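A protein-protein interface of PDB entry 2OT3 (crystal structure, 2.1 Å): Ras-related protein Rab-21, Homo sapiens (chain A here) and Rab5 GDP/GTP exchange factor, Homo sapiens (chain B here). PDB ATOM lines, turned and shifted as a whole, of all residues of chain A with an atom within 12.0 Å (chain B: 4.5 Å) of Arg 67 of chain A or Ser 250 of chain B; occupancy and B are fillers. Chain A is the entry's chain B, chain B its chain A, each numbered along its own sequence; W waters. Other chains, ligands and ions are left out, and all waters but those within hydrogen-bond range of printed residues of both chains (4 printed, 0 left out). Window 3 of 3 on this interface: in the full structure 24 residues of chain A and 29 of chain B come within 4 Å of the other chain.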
ATOM      1  N   GLY A  13      20.375   4.721 -11.751  1.00  0.00           N
ATOM      2  CA  GLY A  13      21.058   3.609 -12.390  1.00  0.00           C
ATOM      3  C   GLY A  13      22.446   4.054 -12.851  1.00  0.00           C
ATOM      4  O   GLY A  13      22.674   5.231 -13.097  1.00  0.00           O
ATOM      5  N   GLU A  14      23.383   3.121 -12.933  1.00  0.00           N
ATOM      6  CA  GLU A  14      24.637   3.392 -13.634  1.00  0.00           C
ATOM      7  C   GLU A  14      24.419   3.329 -15.137  1.00  0.00           C
ATOM      8  O   GLU A  14      23.514   2.661 -15.608  1.00  0.00           O
ATOM      9  CB  GLU A  14      25.733   2.402 -13.240  1.00  0.00           C
ATOM     10  CG  GLU A  14      26.369   2.669 -11.899  1.00  0.00           C
ATOM     11  CD  GLU A  14      27.462   1.647 -11.568  1.00  0.00           C
ATOM     12  OE1 GLU A  14      27.226   0.422 -11.720  1.00  0.00           O
ATOM     13  OE2 GLU A  14      28.567   2.079 -11.180  1.00  0.00           O
ATOM     14  N   GLY A  15      25.258   4.047 -15.878  1.00  0.00           N
ATOM     15  CA  GLY A  15      25.278   4.015 -17.339  1.00  0.00           C
ATOM     16  C   GLY A  15      25.171   2.649 -17.973  1.00  0.00           C
ATOM     17  O   GLY A  15      24.480   2.487 -18.992  1.00  0.00           O
ATOM     18  N   LYS A  19      20.147   2.991 -18.891  1.00  0.00           N
ATOM     19  CA  LYS A  19      19.173   4.040 -18.557  1.00  0.00           C
ATOM     20  C   LYS A  19      19.112   5.185 -19.581  1.00  0.00           C
ATOM     21  O   LYS A  19      18.043   5.782 -19.798  1.00  0.00           O
ATOM     22  CB  LYS A  19      19.458   4.649 -17.175  1.00  0.00           C
ATOM     23  CG  LYS A  19      20.796   5.378 -17.062  1.00  0.00           C
ATOM     24  CD  LYS A  19      20.836   6.299 -15.827  1.00  0.00           C
ATOM     25  CE  LYS A  19      22.221   6.874 -15.649  1.00  0.00           C
ATOM     26  NZ  LYS A  19      22.321   7.595 -14.370  1.00  0.00           N
ATOM     27  N   THR A  62      20.347  11.174 -12.447  1.00  0.00           N
ATOM     28  CA  THR A  62      21.208  11.271 -11.263  1.00  0.00           C
ATOM     29  C   THR A  62      22.464  10.370 -11.415  1.00  0.00           C
ATOM     30  O   THR A  62      22.386   9.288 -11.967  1.00  0.00           O
ATOM     31  CB  THR A  62      20.406  10.948  -9.951  1.00  0.00           C
ATOM     32  OG1 THR A  62      20.063   9.558  -9.920  1.00  0.00           O
ATOM     33  CG2 THR A  62      19.107  11.768  -9.889  1.00  0.00           C
ATOM     34  N   ALA A  63      23.617  10.853 -10.969  1.00  0.00           N
ATOM     35  CA  ALA A  63      24.892  10.150 -11.165  1.00  0.00           C
ATOM     36  C   ALA A  63      24.872   8.841 -10.372  1.00  0.00           C
ATOM     37  O   ALA A  63      24.695   8.875  -9.156  1.00  0.00           O
ATOM     38  CB  ALA A  63      26.056  11.011 -10.701  1.00  0.00           C
ATOM     39  N   GLY A  64      25.054   7.720 -11.063  1.00  0.00           N
ATOM     40  CA  GLY A  64      24.898   6.396 -10.446  1.00  0.00           C
ATOM     41  C   GLY A  64      26.139   5.754  -9.852  1.00  0.00           C
ATOM     42  O   GLY A  64      26.039   4.713  -9.178  1.00  0.00           O
ATOM     43  N   GLN A  65      27.307   6.342 -10.115  1.00  0.00           N
ATOM     44  CA  GLN A  65      28.567   5.799  -9.607  1.00  0.00           C
ATOM     45  C   GLN A  65      28.611   5.793  -8.082  1.00  0.00           C
ATOM     46  O   GLN A  65      28.124   6.716  -7.419  1.00  0.00           O
ATOM     47  CB  GLN A  65      29.768   6.566 -10.159  1.00  0.00           C
ATOM     48  CG  GLN A  65      29.931   6.457 -11.675  1.00  0.00           C
ATOM     49  CD  GLN A  65      30.856   7.525 -12.236  1.00  0.00           C
ATOM     50  OE1 GLN A  65      32.079   7.422 -12.088  1.00  0.00           O
ATOM     51  NE2 GLN A  65      30.281   8.573 -12.878  1.00  0.00           N
ATOM     52  N   GLU A  66      29.248   4.763  -7.548  1.00  0.00           N
ATOM     53  CA  GLU A  66      29.438   4.616  -6.118  1.00  0.00           C
ATOM     54  C   GLU A  66      30.058   5.825  -5.410  1.00  0.00           C
ATOM     55  O   GLU A  66      29.587   6.204  -4.339  1.00  0.00           O
ATOM     56  CB  GLU A  66      30.228   3.327  -5.830  1.00  0.00           C
ATOM     57  CG  GLU A  66      30.718   3.193  -4.396  1.00  0.00           C
ATOM     58  CD  GLU A  66      29.579   3.134  -3.383  1.00  0.00           C
ATOM     59  OE1 GLU A  66      28.477   2.627  -3.736  1.00  0.00           O
ATOM     60  OE2 GLU A  66      29.798   3.585  -2.230  1.00  0.00           O
ATOM     61  N   ARG A  67      31.079   6.444  -6.007  1.00  0.00           N
ATOM     62  CA  ARG A  67      31.690   7.680  -5.457  1.00  0.00           C
ATOM     63  C   ARG A  67      30.695   8.830  -5.202  1.00  0.00           C
ATOM     64  O   ARG A  67      30.983   9.744  -4.420  1.00  0.00           O
ATOM     65  CB  ARG A  67      32.833   8.183  -6.345  1.00  0.00           C
ATOM     66  CG  ARG A  67      32.421   8.495  -7.787  1.00  0.00           C
ATOM     67  CD  ARG A  67      33.569   9.052  -8.640  1.00  0.00           C
ATOM     68  NE  ARG A  67      33.211   9.073 -10.063  1.00  0.00           N
ATOM     69  CZ  ARG A  67      33.699   9.919 -10.978  1.00  0.00           C
ATOM     70  NH1 ARG A  67      34.576  10.865 -10.655  1.00  0.00           N
ATOM     71  NH2 ARG A  67      33.289   9.829 -12.234  1.00  0.00           N
ATOM     72  N   PHE A  68      29.537   8.785  -5.864  1.00  0.00           N
ATOM     73  CA  PHE A  68      28.509   9.817  -5.678  1.00  0.00           C
ATOM     74  C   PHE A  68      27.366   9.373  -4.779  1.00  0.00           C
ATOM     75  O   PHE A  68      26.305  10.014  -4.754  1.00  0.00           O
ATOM     76  CB  PHE A  68      27.969  10.297  -7.030  1.00  0.00           C
ATOM     77  CG  PHE A  68      29.027  10.846  -7.923  1.00  0.00           C
ATOM     78  CD1 PHE A  68      29.928  11.814  -7.447  1.00  0.00           C
ATOM     79  CD2 PHE A  68      29.151  10.394  -9.221  1.00  0.00           C
ATOM     80  CE1 PHE A  68      30.943  12.319  -8.278  1.00  0.00           C
ATOM     81  CE2 PHE A  68      30.146  10.903 -10.058  1.00  0.00           C
ATOM     82  CZ  PHE A  68      31.047  11.859  -9.588  1.00  0.00           C
ATOM     83  N   HIS A  69      27.589   8.308  -4.010  1.00  0.00           N
ATOM     84  CA  HIS A  69      26.497   7.714  -3.236  1.00  0.00           C
ATOM     85  C   HIS A  69      25.827   8.643  -2.219  1.00  0.00           C
ATOM     86  O   HIS A  69      24.621   8.604  -2.062  1.00  0.00           O
ATOM     87  CB  HIS A  69      26.910   6.399  -2.558  1.00  0.00           C
ATOM     88  CG  HIS A  69      25.809   5.802  -1.731  1.00  0.00           C
ATOM     89  ND1 HIS A  69      24.550   5.543  -2.244  1.00  0.00           N
ATOM     90  CD2 HIS A  69      25.764   5.445  -0.423  1.00  0.00           C
ATOM     91  CE1 HIS A  69      23.785   5.042  -1.288  1.00  0.00           C
ATOM     92  NE2 HIS A  69      24.497   4.969  -0.175  1.00  0.00           N
ATOM     93  N   ALA A  70      26.593   9.512  -1.568  1.00  0.00           N
ATOM     94  CA  ALA A  70      26.035  10.383  -0.540  1.00  0.00           C
ATOM     95  C   ALA A  70      25.209  11.554  -1.097  1.00  0.00           C
ATOM     96  O   ALA A  70      24.557  12.273  -0.322  1.00  0.00           O
ATOM     97  CB  ALA A  70      27.146  10.908   0.372  1.00  0.00           C
ATOM     98  N   LEU A  71      25.220  11.738  -2.424  1.00  0.00           N
ATOM     99  CA  LEU A  71      24.612  12.921  -3.064  1.00  0.00           C
ATOM    100  C   LEU A  71      23.150  12.752  -3.459  1.00  0.00           C
ATOM    101  O   LEU A  71      22.450  13.739  -3.765  1.00  0.00           O
ATOM    102  CB  LEU A  71      25.419  13.316  -4.314  1.00  0.00           C
ATOM    103  CG  LEU A  71      26.937  13.383  -4.106  1.00  0.00           C
ATOM    104  CD1 LEU A  71      27.656  13.758  -5.355  1.00  0.00           C
ATOM    105  CD2 LEU A  71      27.274  14.349  -2.968  1.00  0.00           C
ATOM    106  N   GLY A  72      22.702  11.504  -3.503  1.00  0.00           N
ATOM    107  CA  GLY A  72      21.333  11.153  -3.898  1.00  0.00           C
ATOM    108  C   GLY A  72      20.257  12.086  -3.391  1.00  0.00           C
ATOM    109  O   GLY A  72      19.540  12.668  -4.187  1.00  0.00           O
ATOM    110  N   PRO A  73      20.118  12.218  -2.064  1.00  0.00           N
ATOM    111  CA  PRO A  73      19.150  13.105  -1.410  1.00  0.00           C
ATOM    112  C   PRO A  73      19.067  14.514  -1.995  1.00  0.00           C
ATOM    113  O   PRO A  73      17.959  15.059  -2.137  1.00  0.00           O
ATOM    114  CB  PRO A  73      19.665  13.162   0.034  1.00  0.00           C
ATOM    115  CG  PRO A  73      20.283  11.833   0.247  1.00  0.00           C
ATOM    116  CD  PRO A  73      20.894  11.443  -1.077  1.00  0.00           C
ATOM    117  N   ILE A  74      20.215  15.101  -2.333  1.00  0.00           N
ATOM    118  CA  ILE A  74      20.261  16.435  -2.964  1.00  0.00           C
ATOM    119  C   ILE A  74      19.480  16.404  -4.264  1.00  0.00           C
ATOM    120  O   ILE A  74      18.627  17.253  -4.495  1.00  0.00           O
ATOM    121  CB  ILE A  74      21.726  16.944  -3.181  1.00  0.00           C
ATOM    122  CG1 ILE A  74      22.514  16.853  -1.864  1.00  0.00           C
ATOM    123  CG2 ILE A  74      21.717  18.393  -3.787  1.00  0.00           C
ATOM    124  CD1 ILE A  74      23.985  17.285  -1.938  1.00  0.00           C
ATOM    125  N   TYR A  75      19.748  15.403  -5.104  1.00  0.00           N
ATOM    126  CA  TYR A  75      18.965  15.202  -6.313  1.00  0.00           C
ATOM    127  C   TYR A  75      17.479  14.875  -6.059  1.00  0.00           C
ATOM    128  O   TYR A  75      16.587  15.365  -6.774  1.00  0.00           O
ATOM    129  CB  TYR A  75      19.491  13.995  -7.052  1.00  0.00           C
ATOM    130  CG  TYR A  75      20.736  14.112  -7.897  1.00  0.00           C
ATOM    131  CD1 TYR A  75      20.741  14.874  -9.066  1.00  0.00           C
ATOM    132  CD2 TYR A  75      21.871  13.343  -7.584  1.00  0.00           C
ATOM    133  CE1 TYR A  75      21.885  14.921  -9.887  1.00  0.00           C
ATOM    134  CE2 TYR A  75      23.007  13.367  -8.390  1.00  0.00           C
ATOM    135  CZ  TYR A  75      23.003  14.153  -9.549  1.00  0.00           C
ATOM    136  OH  TYR A  75      24.109  14.169 -10.357  1.00  0.00           O
ATOM    137  N   TYR A  76      17.212  14.005  -5.075  1.00  0.00           N
ATOM    138  CA  TYR A  76      15.858  13.419  -4.926  1.00  0.00           C
ATOM    139  C   TYR A  76      14.821  14.378  -4.336  1.00  0.00           C
ATOM    140  O   TYR A  76      13.623  14.162  -4.485  1.00  0.00           O
ATOM    141  CB  TYR A  76      15.885  12.153  -4.056  1.00  0.00           C
ATOM    142  CG  TYR A  76      16.904  11.110  -4.435  1.00  0.00           C
ATOM    143  CD1 TYR A  76      17.301  10.927  -5.765  1.00  0.00           C
ATOM    144  CD2 TYR A  76      17.461  10.288  -3.455  1.00  0.00           C
ATOM    145  CE1 TYR A  76      18.227   9.956  -6.105  1.00  0.00           C
ATOM    146  CE2 TYR A  76      18.374   9.318  -3.777  1.00  0.00           C
ATOM    147  CZ  TYR A  76      18.758   9.150  -5.084  1.00  0.00           C
ATOM    148  OH  TYR A  76      19.691   8.187  -5.388  1.00  0.00           O
ATOM    149  N   LYS A  96      21.418  -2.748  -6.019  1.00  0.00           N
ATOM    150  CA  LYS A  96      21.533  -1.285  -5.953  1.00  0.00           C
ATOM    151  C   LYS A  96      20.186  -0.585  -5.881  1.00  0.00           C
ATOM    152  O   LYS A  96      20.049   0.390  -5.163  1.00  0.00           O
ATOM    153  CB  LYS A  96      22.304  -0.743  -7.152  1.00  0.00           C
ATOM    154  CG  LYS A  96      23.811  -0.968  -7.054  1.00  0.00           C
ATOM    155  CD  LYS A  96      24.555  -0.174  -8.132  1.00  0.00           C
ATOM    156  CE  LYS A  96      26.048  -0.176  -7.887  1.00  0.00           C
ATOM    157  NZ  LYS A  96      26.573  -1.577  -7.790  1.00  0.00           N
ATOM    158  N   TRP A 100      18.643   2.177  -3.129  1.00  0.00           N
ATOM    159  CA  TRP A 100      18.073   3.456  -3.615  1.00  0.00           C
ATOM    160  C   TRP A 100      16.638   3.689  -3.131  1.00  0.00           C
ATOM    161  O   TRP A 100      16.271   4.806  -2.719  1.00  0.00           O
ATOM    162  CB  TRP A 100      18.159   3.543  -5.147  1.00  0.00           C
ATOM    163  CG  TRP A 100      19.541   3.885  -5.663  1.00  0.00           C
ATOM    164  CD1 TRP A 100      20.459   4.725  -5.076  1.00  0.00           C
ATOM    165  CD2 TRP A 100      20.141   3.432  -6.896  1.00  0.00           C
ATOM    166  NE1 TRP A 100      21.599   4.805  -5.864  1.00  0.00           N
ATOM    167  CE2 TRP A 100      21.425   4.029  -6.983  1.00  0.00           C
ATOM    168  CE3 TRP A 100      19.711   2.594  -7.936  1.00  0.00           C
ATOM    169  CZ2 TRP A 100      22.297   3.790  -8.063  1.00  0.00           C
ATOM    170  CZ3 TRP A 100      20.577   2.359  -9.015  1.00  0.00           C
ATOM    171  CH2 TRP A 100      21.858   2.943  -9.056  1.00  0.00           C
ATOM    172  N   GLU A 103      16.590   5.014   0.353  1.00  0.00           N
ATOM    173  CA  GLU A 103      16.878   6.457   0.350  1.00  0.00           C
ATOM    174  C   GLU A 103      15.671   7.293  -0.071  1.00  0.00           C
ATOM    175  O   GLU A 103      15.339   8.296   0.575  1.00  0.00           O
ATOM    176  CB  GLU A 103      18.061   6.790  -0.574  1.00  0.00           C
ATOM    177  CG  GLU A 103      19.363   6.251  -0.098  1.00  0.00           C
ATOM    178  CD  GLU A 103      20.548   6.804  -0.866  1.00  0.00           C
ATOM    179  OE1 GLU A 103      21.125   6.058  -1.692  1.00  0.00           O
ATOM    180  OE2 GLU A 103      20.907   7.982  -0.648  1.00  0.00           O
ATOM    181  N   LEU B 130      39.126  12.247 -11.728  1.00  0.00           N
ATOM    182  CA  LEU B 130      37.672  12.358 -11.647  1.00  0.00           C
ATOM    183  C   LEU B 130      36.972  11.630 -12.800  1.00  0.00           C
ATOM    184  O   LEU B 130      35.746  11.657 -12.913  1.00  0.00           O
ATOM    185  CB  LEU B 130      37.268  13.837 -11.635  1.00  0.00           C
ATOM    186  CG  LEU B 130      37.694  14.548 -10.355  1.00  0.00           C
ATOM    187  CD1 LEU B 130      37.861  16.050 -10.577  1.00  0.00           C
ATOM    188  CD2 LEU B 130      36.672  14.229  -9.264  1.00  0.00           C
ATOM    189  N   CYS B 131      37.760  10.990 -13.660  1.00  0.00           N
ATOM    190  CA  CYS B 131      37.248  10.329 -14.867  1.00  0.00           C
ATOM    191  C   CYS B 131      36.388  11.284 -15.720  1.00  0.00           C
ATOM    192  O   CYS B 131      35.288  10.936 -16.175  1.00  0.00           O
ATOM    193  CB  CYS B 131      36.450   9.078 -14.484  1.00  0.00           C
ATOM    194  SG  CYS B 131      37.382   7.861 -13.452  1.00  0.00           S
ATOM    195  N   PRO B 194      30.947  14.730 -12.659  1.00  0.00           N
ATOM    196  CA  PRO B 194      32.404  14.862 -12.470  1.00  0.00           C
ATOM    197  C   PRO B 194      33.012  16.004 -13.284  1.00  0.00           C
ATOM    198  O   PRO B 194      33.989  16.614 -12.856  1.00  0.00           O
ATOM    199  CB  PRO B 194      32.977  13.522 -12.987  1.00  0.00           C
ATOM    200  CG  PRO B 194      31.906  12.846 -13.689  1.00  0.00           C
ATOM    201  CD  PRO B 194      30.579  13.424 -13.253  1.00  0.00           C
ATOM    202  N   PHE B 242      30.202  17.033  -2.877  1.00  0.00           N
ATOM    203  CA  PHE B 242      31.267  16.053  -3.216  1.00  0.00           C
ATOM    204  C   PHE B 242      32.656  16.572  -2.888  1.00  0.00           C
ATOM    205  O   PHE B 242      33.482  15.859  -2.302  1.00  0.00           O
ATOM    206  CB  PHE B 242      31.210  15.648  -4.682  1.00  0.00           C
ATOM    207  CG  PHE B 242      32.290  14.657  -5.096  1.00  0.00           C
ATOM    208  CD1 PHE B 242      32.108  13.292  -4.914  1.00  0.00           C
ATOM    209  CD2 PHE B 242      33.485  15.101  -5.669  1.00  0.00           C
ATOM    210  CE1 PHE B 242      33.091  12.391  -5.310  1.00  0.00           C
ATOM    211  CE2 PHE B 242      34.471  14.209  -6.072  1.00  0.00           C
ATOM    212  CZ  PHE B 242      34.274  12.847  -5.895  1.00  0.00           C
ATOM    213  N   LEU B 246      35.307  14.801  -0.332  1.00  0.00           N
ATOM    214  CA  LEU B 246      36.211  14.082  -1.221  1.00  0.00           C
ATOM    215  C   LEU B 246      37.369  13.462  -0.404  1.00  0.00           C
ATOM    216  O   LEU B 246      37.962  14.132   0.427  1.00  0.00           O
ATOM    217  CB  LEU B 246      36.745  15.083  -2.253  1.00  0.00           C
ATOM    218  CG  LEU B 246      37.661  14.748  -3.413  1.00  0.00           C
ATOM    219  CD1 LEU B 246      37.468  15.788  -4.509  1.00  0.00           C
ATOM    220  CD2 LEU B 246      39.124  14.708  -2.957  1.00  0.00           C
ATOM    221  N   ASP B 247      37.663  12.187  -0.640  1.00  0.00           N
ATOM    222  CA  ASP B 247      38.758  11.500   0.067  1.00  0.00           C
ATOM    223  C   ASP B 247      39.555  10.653  -0.908  1.00  0.00           C
ATOM    224  O   ASP B 247      39.274  10.666  -2.099  1.00  0.00           O
ATOM    225  CB  ASP B 247      38.206  10.659   1.244  1.00  0.00           C
ATOM    226  CG  ASP B 247      37.276   9.545   0.795  1.00  0.00           C
ATOM    227  OD1 ASP B 247      37.347   9.087  -0.361  1.00  0.00           O
ATOM    228  OD2 ASP B 247      36.469   9.091   1.622  1.00  0.00           O
ATOM    229  N   ALA B 248      40.558   9.926  -0.421  1.00  0.00           N
ATOM    230  CA  ALA B 248      41.414   9.112  -1.302  1.00  0.00           C
ATOM    231  C   ALA B 248      40.594   8.154  -2.168  1.00  0.00           C
ATOM    232  O   ALA B 248      40.859   7.982  -3.365  1.00  0.00           O
ATOM    233  CB  ALA B 248      42.427   8.337  -0.467  1.00  0.00           C
ATOM    234  N   GLN B 249      39.606   7.523  -1.536  1.00  0.00           N
ATOM    235  CA  GLN B 249      38.745   6.533  -2.189  1.00  0.00           C
ATOM    236  C   GLN B 249      37.918   7.157  -3.333  1.00  0.00           C
ATOM    237  O   GLN B 249      37.809   6.568  -4.410  1.00  0.00           O
ATOM    238  CB  GLN B 249      37.847   5.832  -1.141  1.00  0.00           C
ATOM    239  CG  GLN B 249      38.599   4.952  -0.078  1.00  0.00           C
ATOM    240  CD  GLN B 249      39.538   5.728   0.890  1.00  0.00           C
ATOM    241  OE1 GLN B 249      39.266   6.872   1.300  1.00  0.00           O
ATOM    242  NE2 GLN B 249      40.655   5.078   1.266  1.00  0.00           N
ATOM    243  N   SER B 250      37.390   8.366  -3.112  1.00  0.00           N
ATOM    244  CA  SER B 250      36.717   9.164  -4.180  1.00  0.00           C
ATOM    245  C   SER B 250      37.458   9.192  -5.512  1.00  0.00           C
ATOM    246  O   SER B 250      36.849   9.091  -6.588  1.00  0.00           O
ATOM    247  CB  SER B 250      36.535  10.601  -3.709  1.00  0.00           C
ATOM    248  OG  SER B 250      35.873  10.593  -2.473  1.00  0.00           O
ATOM    249  N   LEU B 251      38.780   9.319  -5.430  1.00  0.00           N
ATOM    250  CA  LEU B 251      39.621   9.461  -6.592  1.00  0.00           C
ATOM    251  C   LEU B 251      40.408   8.187  -6.953  1.00  0.00           C
ATOM    252  O   LEU B 251      41.357   8.225  -7.751  1.00  0.00           O
ATOM    253  CB  LEU B 251      40.578  10.624  -6.379  1.00  0.00           C
ATOM    254  CG  LEU B 251      39.956  11.954  -5.971  1.00  0.00           C
ATOM    255  CD1 LEU B 251      41.066  12.946  -5.628  1.00  0.00           C
ATOM    256  CD2 LEU B 251      39.044  12.488  -7.085  1.00  0.00           C
ATOM    257  N   ASN B 252      40.001   7.060  -6.390  1.00  0.00           N
ATOM    258  CA  ASN B 252      40.704   5.807  -6.630  1.00  0.00           C
ATOM    259  C   ASN B 252      42.195   5.909  -6.274  1.00  0.00           C
ATOM    260  O   ASN B 252      43.047   5.387  -7.005  1.00  0.00           O
ATOM    261  CB  ASN B 252      40.522   5.364  -8.097  1.00  0.00           C
ATOM    262  CG  ASN B 252      39.049   5.342  -8.537  1.00  0.00           C
ATOM    263  OD1 ASN B 252      38.192   4.746  -7.871  1.00  0.00           O
ATOM    264  ND2 ASN B 252      38.758   5.985  -9.675  1.00  0.00           N
HETATM  265  O   HOH W   1      32.892   9.723 -15.247  1.00  0.00           O
HETATM  266  O   HOH W   2      32.952  10.599  -2.164  1.00  0.00           O
HETATM  267  O   HOH W   3      34.552   5.973 -12.069  1.00  0.00           O
HETATM  268  O   HOH W   4      36.851   9.852  -9.440  1.00  0.00           O
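Cys 131 of chain B touches Arg 67 of chain A. NH2 of Arg 67 of chain A touches CG of Pro 194 of chain B, 3.6 Å away. Phe 242 of chain B touches Arg 67 of chain A. Arg 67 of chain A touches Ser 250 of chain B (CD to O, 3.9 Å). Phe 68 of chain A touches Phe 242 of chain B (CD1 to CD1, 3.7 Å). CD2 of Leu 71 of chain A touches N of Phe 242 of chain B (3.97 Å).
Of chain B, only Leu 130, Cys 131, Pro 194, Phe 242 and Ser 250 come within 4 Å of Arg 67 of chain A. Ser 250 of chain B touches just one residue of chain A: Arg 67. Printed residues of chain A within 4 Å of Phe 242 of chain B: Arg 67, Phe 68 and Leu 71. No residue of chain A comes within 4 Å of Leu 246 of chain B. Asp 247 of chain B touches none of the printed residues of chain A. No residue of chain A comes within 4 Å of Ala 248 of chain B. Gln 249 of chain B touches none of the printed residues of chain A. No residue of chain A comes within 4 Å of Leu 251 of chain B. No residue of chain A comes within 4 Å of Asn 252 of chain B. Printed residues of chain A within 4 Å of Pro 194 of chain B: Arg 67. Of the printed residues of chain B, Phe 68 of chain A touches Phe 242 (3.7 Å). Of the printed residues of chain B, Leu 71 of chain A touches Phe 242 (3.97 Å). Ala 70 of chain A touches none of the printed residues of chain B. The nearest printed residue of chain B that does not touch Arg 67 of chain A is Gln 249 of chain B (5.6 Å). The nearest residue of chain A that does not touch Ser 250 of chain B is Phe 68 of chain A (6.9 Å).
Of the 22 printed residues of chain A, 3 touch a printed residue of chain B. Printed residues of chain A that touch a printed residue of chain B: Arg 67, Phe 68 and Leu 71. Printed residues of chain B that touch a printed residue of chain A: Leu 130, Cys 131, Pro 194, Phe 242 and Ser 250. Hydrophobic or aromatic side chains of chain B that line the printed part of chain A: Pro 194 and Phe 242. Among the printed residues, 7 pairs touch across the chains. Among the printed residues, no Asp or Glu carboxylate lies within 4 Å of a Lys or Arg side-chain nitrogen of the other chain.
Water W4 lies within hydrogen-bond range of the guanidinium group (NH1) of Arg 67 of chain A and the backbone carbonyl oxygen (O) of Ser 250 of chain B. Water W1 lies within hydrogen-bond range of O of Cys 131 of chain B (2.8 Å) and NH2 of Arg 67 of chain A (3.0 Å). Water W3 lies within hydrogen-bond range of the side-chain amide oxygen (OE1) of Gln 65 of chain A (2.9 Å) and the side-chain sulfur (SG) of Cys 131 of chain B (3.7 Å). Water W2 bridges OG of Ser 250 of chain B (2.9 Å) and O of Arg 67 of chain A (3.1 Å).
O of Leu 130 of chain B is in hydrogen-bond range of NH1 of Arg 67 of chain A (2.7 Å).
OD1 of Asp 247 of chain B sits at hydrogen-bond distance from N of Ser 250 of chain B (2.8 Å). NH2 of Arg 67 of chain A sits at hydrogen-bond distance from OE1 of Gln 65 of chain A (2.7 Å).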
